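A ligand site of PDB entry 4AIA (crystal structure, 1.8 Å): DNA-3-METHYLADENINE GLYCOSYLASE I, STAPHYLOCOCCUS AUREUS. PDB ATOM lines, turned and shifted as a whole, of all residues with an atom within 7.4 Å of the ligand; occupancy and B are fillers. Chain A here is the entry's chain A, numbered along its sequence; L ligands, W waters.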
ATOM      1  N   PHE A   8       2.681 -14.014   8.222  1.00  0.00           N
ATOM      2  CA  PHE A   8       1.624 -13.428   9.072  1.00  0.00           C
ATOM      3  C   PHE A   8       2.115 -12.187   9.827  1.00  0.00           C
ATOM      4  O   PHE A   8       1.722 -11.913  10.965  1.00  0.00           O
ATOM      5  CB  PHE A   8       1.008 -14.524   9.962  1.00  0.00           C
ATOM      6  CG  PHE A   8       0.692 -15.797   9.201  1.00  0.00           C
ATOM      7  CD1 PHE A   8      -0.466 -15.908   8.445  1.00  0.00           C
ATOM      8  CD2 PHE A   8       1.615 -16.849   9.161  1.00  0.00           C
ATOM      9  CE1 PHE A   8      -0.730 -17.053   7.698  1.00  0.00           C
ATOM     10  CE2 PHE A   8       1.365 -17.992   8.423  1.00  0.00           C
ATOM     11  CZ  PHE A   8       0.181 -18.098   7.688  1.00  0.00           C
ATOM     12  N   TYR A  15       8.222 -17.717  15.995  1.00  0.00           N
ATOM     13  CA  TYR A  15       7.276 -17.907  14.923  1.00  0.00           C
ATOM     14  C   TYR A  15       8.049 -17.968  13.607  1.00  0.00           C
ATOM     15  O   TYR A  15       7.742 -18.785  12.751  1.00  0.00           O
ATOM     16  CB  TYR A  15       6.227 -16.783  14.929  1.00  0.00           C
ATOM     17  CG  TYR A  15       4.898 -17.105  14.264  1.00  0.00           C
ATOM     18  CD1 TYR A  15       4.622 -18.360  13.692  1.00  0.00           C
ATOM     19  CD2 TYR A  15       3.880 -16.158  14.260  1.00  0.00           C
ATOM     20  CE1 TYR A  15       3.372 -18.627  13.114  1.00  0.00           C
ATOM     21  CE2 TYR A  15       2.645 -16.412  13.678  1.00  0.00           C
ATOM     22  CZ  TYR A  15       2.398 -17.655  13.101  1.00  0.00           C
ATOM     23  OH  TYR A  15       1.144 -17.897  12.539  1.00  0.00           O
ATOM     24  N   TYR A  18       9.716 -21.396  13.215  1.00  0.00           N
ATOM     25  CA  TYR A  18       8.622 -22.271  12.821  1.00  0.00           C
ATOM     26  C   TYR A  18       8.321 -22.093  11.320  1.00  0.00           C
ATOM     27  O   TYR A  18       8.218 -23.063  10.590  1.00  0.00           O
ATOM     28  CB  TYR A  18       7.368 -21.999  13.672  1.00  0.00           C
ATOM     29  CG  TYR A  18       6.132 -22.725  13.220  1.00  0.00           C
ATOM     30  CD1 TYR A  18       5.956 -24.078  13.525  1.00  0.00           C
ATOM     31  CD2 TYR A  18       5.139 -22.075  12.494  1.00  0.00           C
ATOM     32  CE1 TYR A  18       4.803 -24.765  13.111  1.00  0.00           C
ATOM     33  CE2 TYR A  18       4.008 -22.731  12.062  1.00  0.00           C
ATOM     34  CZ  TYR A  18       3.834 -24.078  12.397  1.00  0.00           C
ATOM     35  OH  TYR A  18       2.703 -24.721  11.962  1.00  0.00           O
ATOM     36  N   HIS A  19       8.192 -20.832  10.869  1.00  0.00           N
ATOM     37  CA  HIS A  19       7.922 -20.563   9.441  1.00  0.00           C
ATOM     38  C   HIS A  19       8.983 -21.153   8.530  1.00  0.00           C
ATOM     39  O   HIS A  19       8.680 -21.734   7.476  1.00  0.00           O
ATOM     40  CB  HIS A  19       7.857 -19.031   9.180  1.00  0.00           C
ATOM     41  CG  HIS A  19       7.277 -18.680   7.829  1.00  0.00           C
ATOM     42  ND1 HIS A  19       5.937 -18.687   7.606  1.00  0.00           N
ATOM     43  CD2 HIS A  19       7.888 -18.374   6.618  1.00  0.00           C
ATOM     44  CE1 HIS A  19       5.692 -18.378   6.321  1.00  0.00           C
ATOM     45  NE2 HIS A  19       6.882 -18.193   5.695  1.00  0.00           N
ATOM     46  N   TRP A  23       6.729 -24.945   8.995  1.00  0.00           N
ATOM     47  CA  TRP A  23       5.519 -24.645   8.226  1.00  0.00           C
ATOM     48  C   TRP A  23       5.744 -24.804   6.732  1.00  0.00           C
ATOM     49  O   TRP A  23       6.671 -24.215   6.150  1.00  0.00           O
ATOM     50  CB  TRP A  23       5.033 -23.242   8.569  1.00  0.00           C
ATOM     51  CG  TRP A  23       3.633 -22.967   8.104  1.00  0.00           C
ATOM     52  CD1 TRP A  23       2.430 -23.414   8.678  1.00  0.00           C
ATOM     53  CD2 TRP A  23       3.237 -22.155   6.960  1.00  0.00           C
ATOM     54  NE1 TRP A  23       1.355 -22.957   7.974  1.00  0.00           N
ATOM     55  CE2 TRP A  23       1.773 -22.167   6.941  1.00  0.00           C
ATOM     56  CE3 TRP A  23       3.924 -21.424   5.992  1.00  0.00           C
ATOM     57  CZ2 TRP A  23       1.045 -21.484   5.966  1.00  0.00           C
ATOM     58  CZ3 TRP A  23       3.189 -20.734   5.016  1.00  0.00           C
ATOM     59  CH2 TRP A  23       1.775 -20.753   5.015  1.00  0.00           C
ATOM     60  N   LEU A  36       1.665 -32.574  14.794  1.00  0.00           N
ATOM     61  CA  LEU A  36       1.215 -31.310  14.191  1.00  0.00           C
ATOM     62  C   LEU A  36      -0.305 -31.282  14.138  1.00  0.00           C
ATOM     63  O   LEU A  36      -0.911 -30.241  14.403  1.00  0.00           O
ATOM     64  CB  LEU A  36       1.748 -31.142  12.757  1.00  0.00           C
ATOM     65  CG  LEU A  36       3.271 -31.020  12.578  1.00  0.00           C
ATOM     66  CD1 LEU A  36       3.513 -30.604  11.118  1.00  0.00           C
ATOM     67  CD2 LEU A  36       3.852 -29.985  13.518  1.00  0.00           C
ATOM     68  N   LEU A  39      -1.803 -30.630  17.637  1.00  0.00           N
ATOM     69  CA  LEU A  39      -1.629 -29.211  17.982  1.00  0.00           C
ATOM     70  C   LEU A  39      -2.621 -28.295  17.216  1.00  0.00           C
ATOM     71  O   LEU A  39      -3.216 -27.377  17.820  1.00  0.00           O
ATOM     72  CB  LEU A  39      -0.179 -28.779  17.781  1.00  0.00           C
ATOM     73  CG  LEU A  39       0.825 -29.314  18.811  1.00  0.00           C
ATOM     74  CD1 LEU A  39       2.246 -29.005  18.370  1.00  0.00           C
ATOM     75  CD2 LEU A  39       0.578 -28.765  20.224  1.00  0.00           C
ATOM     76  N   GLU A  40      -2.838 -28.544  15.922  1.00  0.00           N
ATOM     77  CA  GLU A  40      -3.826 -27.773  15.152  1.00  0.00           C
ATOM     78  C   GLU A  40      -5.223 -27.849  15.762  1.00  0.00           C
ATOM     79  O   GLU A  40      -5.953 -26.856  15.780  1.00  0.00           O
ATOM     80  CB  GLU A  40      -3.895 -28.196  13.666  1.00  0.00           C
ATOM     81  CG  GLU A  40      -2.585 -27.990  12.885  1.00  0.00           C
ATOM     82  CD  GLU A  40      -2.272 -26.522  12.620  1.00  0.00           C
ATOM     83  OE1 GLU A  40      -3.173 -25.679  12.667  1.00  0.00           O
ATOM     84  OE2 GLU A  40      -1.097 -26.224  12.351  1.00  0.00           O
ATOM     85  N   HIS A  43      -6.321 -25.110  18.447  1.00  0.00           N
ATOM     86  CA  HIS A  43      -6.309 -23.686  18.058  1.00  0.00           C
ATOM     87  C   HIS A  43      -7.594 -22.899  18.274  1.00  0.00           C
ATOM     88  O   HIS A  43      -7.553 -21.727  18.685  1.00  0.00           O
ATOM     89  CB  HIS A  43      -5.889 -23.595  16.605  1.00  0.00           C
ATOM     90  CG  HIS A  43      -6.070 -22.224  15.994  1.00  0.00           C
ATOM     91  ND1 HIS A  43      -7.047 -21.948  15.092  1.00  0.00           N
ATOM     92  CD2 HIS A  43      -5.367 -21.052  16.176  1.00  0.00           C
ATOM     93  CE1 HIS A  43      -6.949 -20.635  14.708  1.00  0.00           C
ATOM     94  NE2 HIS A  43      -5.945 -20.087  15.403  1.00  0.00           N
ATOM     95  N   LEU A  46      -8.300 -19.322  19.939  1.00  0.00           N
ATOM     96  CA  LEU A  46      -7.025 -18.766  20.380  1.00  0.00           C
ATOM     97  C   LEU A  46      -6.210 -18.357  19.157  1.00  0.00           C
ATOM     98  O   LEU A  46      -6.601 -18.701  18.034  1.00  0.00           O
ATOM     99  CB  LEU A  46      -6.223 -19.809  21.182  1.00  0.00           C
ATOM    100  CG  LEU A  46      -6.953 -20.328  22.420  1.00  0.00           C
ATOM    101  CD1 LEU A  46      -6.225 -21.535  22.983  1.00  0.00           C
ATOM    102  CD2 LEU A  46      -7.036 -19.218  23.453  1.00  0.00           C
ATOM    103  N   SER A  47      -5.108 -17.634  19.364  1.00  0.00           N
ATOM    104  CA  SER A  47      -4.197 -17.370  18.243  1.00  0.00           C
ATOM    105  C   SER A  47      -3.311 -18.591  17.981  1.00  0.00           C
ATOM    106  O   SER A  47      -3.078 -19.405  18.882  1.00  0.00           O
ATOM    107  CB  SER A  47      -3.344 -16.121  18.491  1.00  0.00           C
ATOM    108  OG  SER A  47      -2.263 -16.405  19.347  1.00  0.00           O
ATOM    109  N   TRP A  48      -2.807 -18.733  16.770  1.00  0.00           N
ATOM    110  CA  TRP A  48      -1.929 -19.879  16.526  1.00  0.00           C
ATOM    111  C   TRP A  48      -0.621 -19.751  17.299  1.00  0.00           C
ATOM    112  O   TRP A  48      -0.092 -20.723  17.832  1.00  0.00           O
ATOM    113  CB  TRP A  48      -1.676 -20.038  15.039  1.00  0.00           C
ATOM    114  CG  TRP A  48      -0.666 -21.117  14.804  1.00  0.00           C
ATOM    115  CD1 TRP A  48       0.635 -20.990  14.324  1.00  0.00           C
ATOM    116  CD2 TRP A  48      -0.804 -22.508  15.185  1.00  0.00           C
ATOM    117  NE1 TRP A  48       1.267 -22.217  14.336  1.00  0.00           N
ATOM    118  CE2 TRP A  48       0.446 -23.169  14.825  1.00  0.00           C
ATOM    119  CE3 TRP A  48      -1.852 -23.280  15.718  1.00  0.00           C
ATOM    120  CZ2 TRP A  48       0.646 -24.535  15.015  1.00  0.00           C
ATOM    121  CZ3 TRP A  48      -1.623 -24.644  15.926  1.00  0.00           C
ATOM    122  CH2 TRP A  48      -0.425 -25.243  15.578  1.00  0.00           C
ATOM    123  N   LEU A  49      -0.071 -18.541  17.372  1.00  0.00           N
ATOM    124  CA  LEU A  49       1.182 -18.372  18.121  1.00  0.00           C
ATOM    125  C   LEU A  49       1.025 -18.793  19.577  1.00  0.00           C
ATOM    126  O   LEU A  49       1.968 -19.340  20.185  1.00  0.00           O
ATOM    127  CB  LEU A  49       1.710 -16.931  18.040  1.00  0.00           C
ATOM    128  CG  LEU A  49       3.129 -16.638  18.571  1.00  0.00           C
ATOM    129  CD1 LEU A  49       4.163 -17.637  18.044  1.00  0.00           C
ATOM    130  CD2 LEU A  49       3.497 -15.213  18.208  1.00  0.00           C
ATOM    131  N   LEU A  52       1.564 -22.471  19.604  1.00  0.00           N
ATOM    132  CA  LEU A  52       2.986 -22.737  19.321  1.00  0.00           C
ATOM    133  C   LEU A  52       3.824 -22.610  20.565  1.00  0.00           C
ATOM    134  O   LEU A  52       4.722 -23.457  20.835  1.00  0.00           O
ATOM    135  CB  LEU A  52       3.536 -21.760  18.285  1.00  0.00           C
ATOM    136  CG  LEU A  52       3.332 -22.099  16.823  1.00  0.00           C
ATOM    137  CD1 LEU A  52       4.166 -21.169  15.960  1.00  0.00           C
ATOM    138  CD2 LEU A  52       3.676 -23.557  16.531  1.00  0.00           C
ATOM    139  N   ARG A 137      -4.700 -16.340  -0.390  1.00  0.00           N
ATOM    140  CA  ARG A 137      -4.858 -17.546   0.427  1.00  0.00           C
ATOM    141  C   ARG A 137      -6.282 -17.900   0.744  1.00  0.00           C
ATOM    142  O   ARG A 137      -7.066 -17.034   1.095  1.00  0.00           O
ATOM    143  CB  ARG A 137      -4.080 -17.399   1.723  1.00  0.00           C
ATOM    144  CG  ARG A 137      -2.581 -17.387   1.485  1.00  0.00           C
ATOM    145  CD  ARG A 137      -1.909 -17.954   2.707  1.00  0.00           C
ATOM    146  NE  ARG A 137      -0.424 -17.974   2.639  1.00  0.00           N
ATOM    147  CZ  ARG A 137       0.370 -17.266   3.441  1.00  0.00           C
ATOM    148  NH1 ARG A 137      -0.150 -16.444   4.354  1.00  0.00           N
ATOM    149  NH2 ARG A 137       1.683 -17.392   3.334  1.00  0.00           N
ATOM    150  N   VAL A 162     -11.632 -26.644   8.025  1.00  0.00           N
ATOM    151  CA  VAL A 162     -10.721 -25.459   8.108  1.00  0.00           C
ATOM    152  C   VAL A 162      -9.461 -25.862   8.882  1.00  0.00           C
ATOM    153  O   VAL A 162      -8.335 -25.558   8.483  1.00  0.00           O
ATOM    154  CB  VAL A 162     -11.429 -24.256   8.779  1.00  0.00           C
ATOM    155  CG1 VAL A 162     -10.464 -23.126   9.114  1.00  0.00           C
ATOM    156  CG2 VAL A 162     -12.524 -23.720   7.877  1.00  0.00           C
ATOM    157  N   THR A 163      -9.655 -26.563   9.995  1.00  0.00           N
ATOM    158  CA  THR A 163      -8.530 -27.024  10.840  1.00  0.00           C
ATOM    159  C   THR A 163      -7.619 -27.986  10.090  1.00  0.00           C
ATOM    160  O   THR A 163      -6.376 -27.899  10.141  1.00  0.00           O
ATOM    161  CB  THR A 163      -9.061 -27.624  12.161  1.00  0.00           C
ATOM    162  OG1 THR A 163      -9.756 -26.581  12.860  1.00  0.00           O
ATOM    163  CG2 THR A 163      -7.917 -28.087  13.076  1.00  0.00           C
ATOM    164  N   SER A 166      -5.506 -26.119   7.577  1.00  0.00           N
ATOM    165  CA  SER A 166      -4.350 -25.553   8.300  1.00  0.00           C
ATOM    166  C   SER A 166      -3.257 -26.565   8.556  1.00  0.00           C
ATOM    167  O   SER A 166      -2.055 -26.258   8.386  1.00  0.00           O
ATOM    168  CB  SER A 166      -4.823 -24.923   9.622  1.00  0.00           C
ATOM    169  OG  SER A 166      -5.602 -23.765   9.357  1.00  0.00           O
ATOM    170  N   PHE A 167      -3.637 -27.773   8.991  1.00  0.00           N
ATOM    171  CA  PHE A 167      -2.691 -28.864   9.130  1.00  0.00           C
ATOM    172  C   PHE A 167      -1.993 -29.222   7.823  1.00  0.00           C
ATOM    173  O   PHE A 167      -0.765 -29.440   7.820  1.00  0.00           O
ATOM    174  CB  PHE A 167      -3.406 -30.128   9.711  1.00  0.00           C
ATOM    175  CG  PHE A 167      -2.612 -31.399   9.506  1.00  0.00           C
ATOM    176  CD1 PHE A 167      -1.506 -31.692  10.320  1.00  0.00           C
ATOM    177  CD2 PHE A 167      -2.953 -32.280   8.490  1.00  0.00           C
ATOM    178  CE1 PHE A 167      -0.768 -32.849  10.129  1.00  0.00           C
ATOM    179  CE2 PHE A 167      -2.217 -33.441   8.279  1.00  0.00           C
ATOM    180  CZ  PHE A 167      -1.117 -33.727   9.093  1.00  0.00           C
ATOM    181  N   GLU A 169      -1.289 -27.374   5.268  1.00  0.00           N
ATOM    182  CA  GLU A 169      -0.270 -26.320   5.032  1.00  0.00           C
ATOM    183  C   GLU A 169       0.919 -26.455   5.985  1.00  0.00           C
ATOM    184  O   GLU A 169       2.082 -26.309   5.562  1.00  0.00           O
ATOM    185  CB  GLU A 169      -0.858 -24.922   5.209  1.00  0.00           C
ATOM    186  CG  GLU A 169      -1.973 -24.532   4.255  1.00  0.00           C
ATOM    187  CD  GLU A 169      -2.552 -23.179   4.654  1.00  0.00           C
ATOM    188  OE1 GLU A 169      -2.950 -23.000   5.820  1.00  0.00           O
ATOM    189  OE2 GLU A 169      -2.641 -22.280   3.819  1.00  0.00           O
ATOM    190  N   ALA A 170       0.633 -26.717   7.257  1.00  0.00           N
ATOM    191  CA  ALA A 170       1.693 -26.823   8.284  1.00  0.00           C
ATOM    192  C   ALA A 170       2.611 -27.988   8.021  1.00  0.00           C
ATOM    193  O   ALA A 170       3.820 -27.852   8.167  1.00  0.00           O
ATOM    194  CB  ALA A 170       1.122 -26.918   9.708  1.00  0.00           C
ATOM    195  N   ALA A 171       2.052 -29.127   7.599  1.00  0.00           N
ATOM    196  CA  ALA A 171       2.789 -30.372   7.362  1.00  0.00           C
ATOM    197  C   ALA A 171       3.496 -30.407   5.974  1.00  0.00           C
ATOM    198  O   ALA A 171       4.242 -31.331   5.647  1.00  0.00           O
ATOM    199  CB  ALA A 171       1.825 -31.555   7.466  1.00  0.00           C
HETATM  200  N1  LIG L   1      -3.531 -20.987  12.071  1.00  0.00           N
HETATM  201  C1  LIG L   1      -2.234 -21.027  11.694  1.00  0.00           C
HETATM  202  N2  LIG L   1      -1.409 -20.053  11.251  1.00  0.00           N
HETATM  203  C2  LIG L   1      -0.106 -20.363  10.934  1.00  0.00           C
HETATM  204  N3  LIG L   1       0.353 -21.599  11.042  1.00  0.00           N
HETATM  205  C3  LIG L   1      -0.507 -22.577  11.497  1.00  0.00           C
HETATM  206  N4  LIG L   1      -0.054 -23.816  11.626  1.00  0.00           N
HETATM  207  C4  LIG L   1      -1.782 -22.280  11.825  1.00  0.00           C
HETATM  208  N5  LIG L   1      -2.803 -23.008  12.296  1.00  0.00           N
HETATM  209  C5  LIG L   1      -3.880 -22.230  12.449  1.00  0.00           C
HETATM  210  C6  LIG L   1      -1.875 -18.640  11.081  1.00  0.00           C
HETATM  211  O   HOH W   1      -5.625 -25.041  13.512  1.00  0.00           O
HETATM  212  O   HOH W   2      -3.660 -21.720   8.863  1.00  0.00           O
HETATM  213  O   HOH W   3      -1.375 -23.505   8.498  1.00  0.00           O
HETATM  214  O   HOH W   4      -5.508 -18.873  11.986  1.00  0.00           O
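O of Tyr 18 lies within hydrogen-bond range of N of Trp 23, at 2.9 Å. OG of Ser 166 lies within hydrogen-bond range of O of Val 162 (3.4 Å).
Merely in contact with the ligand: Phe 8, Tyr 15, Trp 23, Ser 166 and Ala 170. Eight residues have an atom within 4 Å of the ligand: Phe 8, Tyr 15, Tyr 18, Trp 23, Glu 40, Trp 48, Ser 166 and Ala 170. Along chain A the residues within 4 Å of the ligand span positions 8 to 170.
OE1 of Glu 40 is in hydrogen-bond range of N5 of the ligand, at 2.7 Å. OH of Tyr 18 sits at hydrogen-bond distance from N4 of the ligand (2.9 Å). NE1 of Trp 48 sits close to N3 of the ligand (3.5 Å).
Water W2 lies within hydrogen-bond range of the side-chain hydroxyl of Ser 166, a nitrogen (N1) of the ligand and the side-chain carboxylate of Glu 169. Water W3 lies within hydrogen-bond range of NE1 of Trp 23 (2.8 Å), O of Ser 166 (2.8 Å), OE1 of Glu 169 (3.1 Å) and N4 of the ligand (3.4 Å).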
